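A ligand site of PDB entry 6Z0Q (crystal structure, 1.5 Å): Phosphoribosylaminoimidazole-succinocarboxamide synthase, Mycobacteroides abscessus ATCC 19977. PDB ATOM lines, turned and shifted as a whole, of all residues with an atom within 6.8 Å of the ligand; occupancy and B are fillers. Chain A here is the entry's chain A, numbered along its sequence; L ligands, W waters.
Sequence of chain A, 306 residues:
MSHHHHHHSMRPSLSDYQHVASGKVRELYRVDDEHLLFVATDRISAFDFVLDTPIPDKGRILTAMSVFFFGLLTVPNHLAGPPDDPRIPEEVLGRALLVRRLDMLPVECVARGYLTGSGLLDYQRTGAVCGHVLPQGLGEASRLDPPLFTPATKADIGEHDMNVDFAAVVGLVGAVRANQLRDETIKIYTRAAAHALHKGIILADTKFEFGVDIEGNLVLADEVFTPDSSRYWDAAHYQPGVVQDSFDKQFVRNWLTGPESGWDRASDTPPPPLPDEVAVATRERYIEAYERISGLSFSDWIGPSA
Residues that only touch the ligand: Ala 21, Ser 22, Gly 23, Glu 27, Leu 28, Phe 38, Met 104, Leu 105 and Glu 108. Hydrophobic or aromatic side chains that line the ligand: Phe 38 and Met 104. Within 4 Å of the ligand: Ala 21, Ser 22, Gly 23, Arg 26, Glu 27, Leu 28, Phe 38, Met 104, Leu 105, Glu 108 and Glu 209. The nearest printed residue that does not touch the ligand is Val 107 (4.3 Å).
OE1 of Glu 209 is in salt-bridge range of NH2 of Arg 26. The backbone carbonyl oxygen (O) of Glu 209 sits at hydrogen-bond distance from the backbone NH (N) of Ala 221 (3.0 Å). NH1 of Arg 26 lies within salt-bridge range of OD1 of Asp 222. OG of Ser 22 is in hydrogen-bond range of OE1 of Glu 27 (2.8 Å). The side-chain hydroxyl (OG) of Ser 22 is in hydrogen-bond range of a ring nitrogen (NE2) of His 19 (3.1 Å). NE2 of His 19 lies within hydrogen-bond range of OE1 of Glu 27, 2.9 Å away. O of Ala 21 is in hydrogen-bond range of N of Leu 28 (3.0 Å). The backbone carbonyl oxygen (O) of Ala 21 is in hydrogen-bond range of a ring nitrogen (NE2) of His 19 (3.2 Å).
O3 of the ligand is in hydrogen-bond range of OE1 of Glu 209 (2.7 Å). An oxygen (O3) of the ligand sits at hydrogen-bond distance from the guanidinium group (NH2) of Arg 26, 3.5 Å away.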
ATOM      1  N   HIS A  19      12.669 -14.724   9.861  1.00  0.00           N
ATOM      2  CA  HIS A  19      12.203 -14.681   8.486  1.00  0.00           C
ATOM      3  C   HIS A  19      13.063 -13.672   7.735  1.00  0.00           C
ATOM      4  O   HIS A  19      13.101 -12.482   8.088  1.00  0.00           O
ATOM      5  CB  HIS A  19      10.708 -14.296   8.440  1.00  0.00           C
ATOM      6  CG  HIS A  19      10.034 -14.622   7.144  1.00  0.00           C
ATOM      7  ND1 HIS A  19       8.689 -14.366   6.942  1.00  0.00           N
ATOM      8  CD2 HIS A  19      10.489 -15.173   6.002  1.00  0.00           C
ATOM      9  CE1 HIS A  19       8.353 -14.745   5.720  1.00  0.00           C
ATOM     10  NE2 HIS A  19       9.420 -15.236   5.129  1.00  0.00           N
ATOM     11  N   ALA A  21      13.573 -13.619   4.015  1.00  0.00           N
ATOM     12  CA  ALA A  21      13.136 -13.271   2.657  1.00  0.00           C
ATOM     13  C   ALA A  21      11.855 -13.992   2.248  1.00  0.00           C
ATOM     14  O   ALA A  21      11.541 -15.073   2.751  1.00  0.00           O
ATOM     15  CB  ALA A  21      14.251 -13.578   1.648  1.00  0.00           C
ATOM     16  N   SER A  22      11.110 -13.382   1.330  1.00  0.00           N
ATOM     17  CA  SER A  22       9.887 -13.976   0.810  1.00  0.00           C
ATOM     18  C   SER A  22       9.859 -13.902  -0.711  1.00  0.00           C
ATOM     19  O   SER A  22      10.223 -12.888  -1.301  1.00  0.00           O
ATOM     20  CB  SER A  22       8.652 -13.263   1.383  1.00  0.00           C
ATOM     21  OG  SER A  22       8.559 -13.433   2.780  1.00  0.00           O
ATOM     22  N   GLY A  23       9.426 -15.001  -1.345  1.00  0.00           N
ATOM     23  CA  GLY A  23       9.317 -15.076  -2.794  1.00  0.00           C
ATOM     24  C   GLY A  23       7.884 -15.337  -3.222  1.00  0.00           C
ATOM     25  O   GLY A  23       6.984 -15.300  -2.384  1.00  0.00           O
ATOM     26  N   LYS A  24       7.673 -15.627  -4.506  1.00  0.00           N
ATOM     27  CA  LYS A  24       6.321 -15.850  -5.036  1.00  0.00           C
ATOM     28  C   LYS A  24       5.669 -17.078  -4.419  1.00  0.00           C
ATOM     29  O   LYS A  24       4.510 -17.036  -4.007  1.00  0.00           O
ATOM     30  CB  LYS A  24       6.356 -15.990  -6.563  1.00  0.00           C
ATOM     31  N   ARG A  26       7.863 -19.407  -2.423  1.00  0.00           N
ATOM     32  CA  ARG A  26       8.867 -19.927  -1.503  1.00  0.00           C
ATOM     33  C   ARG A  26       9.214 -18.905  -0.404  1.00  0.00           C
ATOM     34  O   ARG A  26       8.972 -17.700  -0.555  1.00  0.00           O
ATOM     35  CB  ARG A  26      10.138 -20.339  -2.274  1.00  0.00           C
ATOM     36  CG  ARG A  26      10.820 -19.227  -3.054  1.00  0.00           C
ATOM     37  CD  ARG A  26      12.104 -19.718  -3.742  1.00  0.00           C
ATOM     38  NE  ARG A  26      12.809 -18.647  -4.450  1.00  0.00           N
ATOM     39  CZ  ARG A  26      14.046 -18.749  -4.926  1.00  0.00           C
ATOM     40  NH1 ARG A  26      14.741 -19.870  -4.765  1.00  0.00           N
ATOM     41  NH2 ARG A  26      14.598 -17.721  -5.563  1.00  0.00           N
ATOM     42  N   GLU A  27       9.784 -19.387   0.704  1.00  0.00           N
ATOM     43  CA  GLU A  27      10.186 -18.538   1.832  1.00  0.00           C
ATOM     44  C   GLU A  27      11.574 -18.921   2.353  1.00  0.00           C
ATOM     45  O   GLU A  27      11.998 -20.062   2.185  1.00  0.00           O
ATOM     46  CB  GLU A  27       9.157 -18.625   2.977  1.00  0.00           C
ATOM     47  CG  GLU A  27       7.702 -18.492   2.521  1.00  0.00           C
ATOM     48  CD  GLU A  27       7.310 -17.047   2.246  1.00  0.00           C
ATOM     49  OE1 GLU A  27       7.988 -16.132   2.754  1.00  0.00           O
ATOM     50  OE2 GLU A  27       6.300 -16.825   1.530  1.00  0.00           O
ATOM     51  N   LEU A  28      12.254 -17.981   3.009  1.00  0.00           N
ATOM     52  CA  LEU A  28      13.610 -18.220   3.507  1.00  0.00           C
ATOM     53  C   LEU A  28      13.755 -17.771   4.969  1.00  0.00           C
ATOM     54  O   LEU A  28      13.338 -16.672   5.325  1.00  0.00           O
ATOM     55  CB  LEU A  28      14.636 -17.499   2.614  1.00  0.00           C
ATOM     56  CG  LEU A  28      16.110 -17.814   2.841  1.00  0.00           C
ATOM     57  CD1 LEU A  28      16.410 -19.273   2.537  1.00  0.00           C
ATOM     58  CD2 LEU A  28      17.007 -16.897   2.012  1.00  0.00           C
ATOM     59  N   PHE A  38      15.246 -23.340   3.708  1.00  0.00           N
ATOM     60  CA  PHE A  38      14.578 -23.099   2.417  1.00  0.00           C
ATOM     61  C   PHE A  38      13.185 -23.743   2.495  1.00  0.00           C
ATOM     62  O   PHE A  38      13.098 -24.961   2.652  1.00  0.00           O
ATOM     63  CB  PHE A  38      15.389 -23.724   1.247  1.00  0.00           C
ATOM     64  CG  PHE A  38      16.259 -22.758   0.444  1.00  0.00           C
ATOM     65  CD1 PHE A  38      17.395 -22.187   0.994  1.00  0.00           C
ATOM     66  CD2 PHE A  38      15.979 -22.516  -0.896  1.00  0.00           C
ATOM     67  CE1 PHE A  38      18.209 -21.329   0.241  1.00  0.00           C
ATOM     68  CE2 PHE A  38      16.777 -21.664  -1.655  1.00  0.00           C
ATOM     69  CZ  PHE A  38      17.897 -21.065  -1.086  1.00  0.00           C
ATOM     70  N   VAL A  39      12.107 -22.970   2.369  1.00  0.00           N
ATOM     71  CA  VAL A  39      10.733 -23.509   2.501  1.00  0.00           C
ATOM     72  C   VAL A  39       9.920 -23.367   1.208  1.00  0.00           C
ATOM     73  O   VAL A  39       9.814 -22.268   0.664  1.00  0.00           O
ATOM     74  CB  VAL A  39       9.967 -22.786   3.640  1.00  0.00           C
ATOM     75  CG1 VAL A  39       8.501 -23.237   3.702  1.00  0.00           C
ATOM     76  CG2 VAL A  39      10.662 -22.987   4.978  1.00  0.00           C
ATOM     77  N   MET A 104      25.845 -15.547  -2.645  1.00  0.00           N
ATOM     78  CA  MET A 104      25.100 -15.838  -3.873  1.00  0.00           C
ATOM     79  C   MET A 104      25.562 -15.007  -5.067  1.00  0.00           C
ATOM     80  O   MET A 104      25.862 -13.814  -4.921  1.00  0.00           O
ATOM     81  CB  MET A 104      23.607 -15.623  -3.635  1.00  0.00           C
ATOM     82  CG  MET A 104      22.997 -16.590  -2.612  1.00  0.00           C
ATOM     83  SD  MET A 104      23.141 -18.349  -3.075  1.00  0.00           S
ATOM     84  CE  MET A 104      22.061 -18.410  -4.497  1.00  0.00           C
ATOM     85  N   LEU A 105      25.606 -15.627  -6.244  1.00  0.00           N
ATOM     86  CA  LEU A 105      25.934 -14.889  -7.475  1.00  0.00           C
ATOM     87  C   LEU A 105      24.660 -14.314  -8.098  1.00  0.00           C
ATOM     88  O   LEU A 105      23.651 -15.019  -8.213  1.00  0.00           O
ATOM     89  CB  LEU A 105      26.667 -15.806  -8.451  1.00  0.00           C
ATOM     90  CG  LEU A 105      27.982 -16.389  -7.913  1.00  0.00           C
ATOM     91  CD1 LEU A 105      28.586 -17.449  -8.830  1.00  0.00           C
ATOM     92  CD2 LEU A 105      28.996 -15.274  -7.646  1.00  0.00           C
ATOM     93  N   PRO A 106      24.677 -13.020  -8.469  1.00  0.00           N
ATOM     94  CA  PRO A 106      23.494 -12.320  -8.968  1.00  0.00           C
ATOM     95  C   PRO A 106      23.219 -12.574 -10.453  1.00  0.00           C
ATOM     96  O   PRO A 106      23.081 -11.630 -11.237  1.00  0.00           O
ATOM     97  CB  PRO A 106      23.824 -10.850  -8.706  1.00  0.00           C
ATOM     98  CG  PRO A 106      25.297 -10.793  -8.847  1.00  0.00           C
ATOM     99  CD  PRO A 106      25.815 -12.095  -8.273  1.00  0.00           C
ATOM    100  N   VAL A 107      23.150 -13.843 -10.819  1.00  0.00           N
ATOM    101  CA  VAL A 107      22.893 -14.247 -12.198  1.00  0.00           C
ATOM    102  C   VAL A 107      21.833 -15.357 -12.216  1.00  0.00           C
ATOM    103  O   VAL A 107      21.979 -16.358 -11.522  1.00  0.00           O
ATOM    104  CB  VAL A 107      24.172 -14.764 -12.900  1.00  0.00           C
ATOM    105  CG1 VAL A 107      23.877 -15.132 -14.356  1.00  0.00           C
ATOM    106  CG2 VAL A 107      25.309 -13.747 -12.817  1.00  0.00           C
ATOM    107  N   GLU A 108      20.759 -15.181 -12.997  1.00  0.00           N
ATOM    108  CA  GLU A 108      19.842 -16.306 -13.236  1.00  0.00           C
ATOM    109  C   GLU A 108      20.409 -17.173 -14.360  1.00  0.00           C
ATOM    110  O   GLU A 108      20.479 -16.731 -15.526  1.00  0.00           O
ATOM    111  CB  GLU A 108      18.430 -15.812 -13.588  1.00  0.00           C
ATOM    112  CG  GLU A 108      17.846 -14.802 -12.604  1.00  0.00           C
ATOM    113  CD  GLU A 108      17.760 -15.335 -11.191  1.00  0.00           C
ATOM    114  OE1 GLU A 108      17.301 -16.486 -11.011  1.00  0.00           O
ATOM    115  OE2 GLU A 108      18.144 -14.599 -10.257  1.00  0.00           O
ATOM    116  N   LYS A 154      17.564 -10.250 -12.467  1.00  0.00           N
ATOM    117  CA  LYS A 154      16.296  -9.868 -11.837  1.00  0.00           C
ATOM    118  C   LYS A 154      16.011  -8.378 -12.040  1.00  0.00           C
ATOM    119  O   LYS A 154      16.909  -7.555 -11.959  1.00  0.00           O
ATOM    120  CB  LYS A 154      16.325 -10.218 -10.354  1.00  0.00           C
ATOM    121  CG  LYS A 154      15.713 -11.559 -10.039  1.00  0.00           C
ATOM    122  CD  LYS A 154      16.064 -12.025  -8.643  1.00  0.00           C
ATOM    123  CE  LYS A 154      15.397 -13.354  -8.332  1.00  0.00           C
ATOM    124  N   PHE A 208      18.733 -22.008 -12.825  1.00  0.00           N
ATOM    125  CA  PHE A 208      19.573 -22.298 -11.655  1.00  0.00           C
ATOM    126  C   PHE A 208      20.007 -21.009 -10.969  1.00  0.00           C
ATOM    127  O   PHE A 208      20.284 -20.020 -11.633  1.00  0.00           O
ATOM    128  CB  PHE A 208      20.884 -23.028 -12.024  1.00  0.00           C
ATOM    129  CG  PHE A 208      20.714 -24.339 -12.714  1.00  0.00           C
ATOM    130  CD1 PHE A 208      19.826 -25.298 -12.247  1.00  0.00           C
ATOM    131  CD2 PHE A 208      21.504 -24.634 -13.808  1.00  0.00           C
ATOM    132  CE1 PHE A 208      19.701 -26.522 -12.902  1.00  0.00           C
ATOM    133  CE2 PHE A 208      21.389 -25.847 -14.465  1.00  0.00           C
ATOM    134  CZ  PHE A 208      20.481 -26.799 -14.005  1.00  0.00           C
ATOM    135  N   GLU A 209      20.141 -21.059  -9.640  1.00  0.00           N
ATOM    136  CA  GLU A 209      20.889 -20.047  -8.905  1.00  0.00           C
ATOM    137  C   GLU A 209      22.057 -20.701  -8.157  1.00  0.00           C
ATOM    138  O   GLU A 209      21.886 -21.744  -7.515  1.00  0.00           O
ATOM    139  CB  GLU A 209      19.948 -19.289  -7.948  1.00  0.00           C
ATOM    140  CG  GLU A 209      18.920 -18.426  -8.706  1.00  0.00           C
ATOM    141  CD  GLU A 209      17.702 -17.990  -7.890  1.00  0.00           C
ATOM    142  OE1 GLU A 209      17.485 -18.485  -6.768  1.00  0.00           O
ATOM    143  OE2 GLU A 209      16.963 -17.112  -8.382  1.00  0.00           O
ATOM    144  N   PHE A 210      23.241 -20.086  -8.238  1.00  0.00           N
ATOM    145  CA  PHE A 210      24.468 -20.608  -7.613  1.00  0.00           C
ATOM    146  C   PHE A 210      25.024 -19.667  -6.541  1.00  0.00           C
ATOM    147  O   PHE A 210      24.852 -18.451  -6.626  1.00  0.00           O
ATOM    148  CB  PHE A 210      25.607 -20.811  -8.632  1.00  0.00           C
ATOM    149  CG  PHE A 210      25.357 -21.868  -9.675  1.00  0.00           C
ATOM    150  CD1 PHE A 210      24.792 -21.532 -10.901  1.00  0.00           C
ATOM    151  CD2 PHE A 210      25.775 -23.181  -9.466  1.00  0.00           C
ATOM    152  CE1 PHE A 210      24.614 -22.513 -11.894  1.00  0.00           C
ATOM    153  CE2 PHE A 210      25.587 -24.173 -10.458  1.00  0.00           C
ATOM    154  CZ  PHE A 210      25.008 -23.830 -11.668  1.00  0.00           C
ATOM    155  N   ALA A 221      22.417 -23.896  -5.457  1.00  0.00           N
ATOM    156  CA  ALA A 221      21.751 -23.365  -4.267  1.00  0.00           C
ATOM    157  C   ALA A 221      20.383 -22.778  -4.550  1.00  0.00           C
ATOM    158  O   ALA A 221      20.197 -21.557  -4.531  1.00  0.00           O
ATOM    159  CB  ALA A 221      22.638 -22.306  -3.604  1.00  0.00           C
ATOM    160  N   ASP A 222      19.421 -23.663  -4.752  1.00  0.00           N
ATOM    161  CA  ASP A 222      18.117 -23.329  -5.274  1.00  0.00           C
ATOM    162  C   ASP A 222      17.294 -24.606  -5.251  1.00  0.00           C
ATOM    163  O   ASP A 222      17.842 -25.695  -5.078  1.00  0.00           O
ATOM    164  CB  ASP A 222      18.264 -22.787  -6.704  1.00  0.00           C
ATOM    165  CG  ASP A 222      17.001 -22.134  -7.239  1.00  0.00           C
ATOM    166  OD1 ASP A 222      16.113 -21.755  -6.449  1.00  0.00           O
ATOM    167  OD2 ASP A 222      16.911 -21.988  -8.482  1.00  0.00           O
HETATM  168  C1  LIG L   1      16.602 -16.708  -2.710  1.00  0.00           C
HETATM  169  C2  LIG L   1      14.120 -16.688  -1.508  1.00  0.00           C
HETATM  170  C3  LIG L   1      14.911 -17.761  -1.428  1.00  0.00           C
HETATM  171  C4  LIG L   1      20.230 -15.080  -7.829  1.00  0.00           C
HETATM  172  C5  LIG L   1      20.660 -15.217  -6.236  1.00  0.00           C
HETATM  173  O1  LIG L   1      19.565 -15.438  -5.494  1.00  0.00           O
HETATM  174  C6  LIG L   1      19.755 -15.076  -4.099  1.00  0.00           C
HETATM  175  O2  LIG L   1      20.472 -14.204  -3.875  1.00  0.00           O
HETATM  176  C7  LIG L   1      19.085 -15.777  -2.950  1.00  0.00           C
HETATM  177  F1  LIG L   1      18.571 -14.855  -2.084  1.00  0.00           F
HETATM  178  C8  LIG L   1      18.039 -16.825  -3.381  1.00  0.00           C
HETATM  179  O3  LIG L   1      17.870 -16.788  -4.761  1.00  0.00           O
HETATM  180  C9  LIG L   1      15.855 -15.611  -2.828  1.00  0.00           C
HETATM  181  C10 LIG L   1      14.587 -15.543  -2.231  1.00  0.00           C
HETATM  182 BR1  LIG L   1      12.407 -16.680  -0.662  1.00  0.00          BR
HETATM  183  N1  LIG L   1      16.107 -17.790  -2.010  1.00  0.00           N
HETATM  184  O   HOH W   1      21.592 -13.391  -1.229  1.00  0.00           O
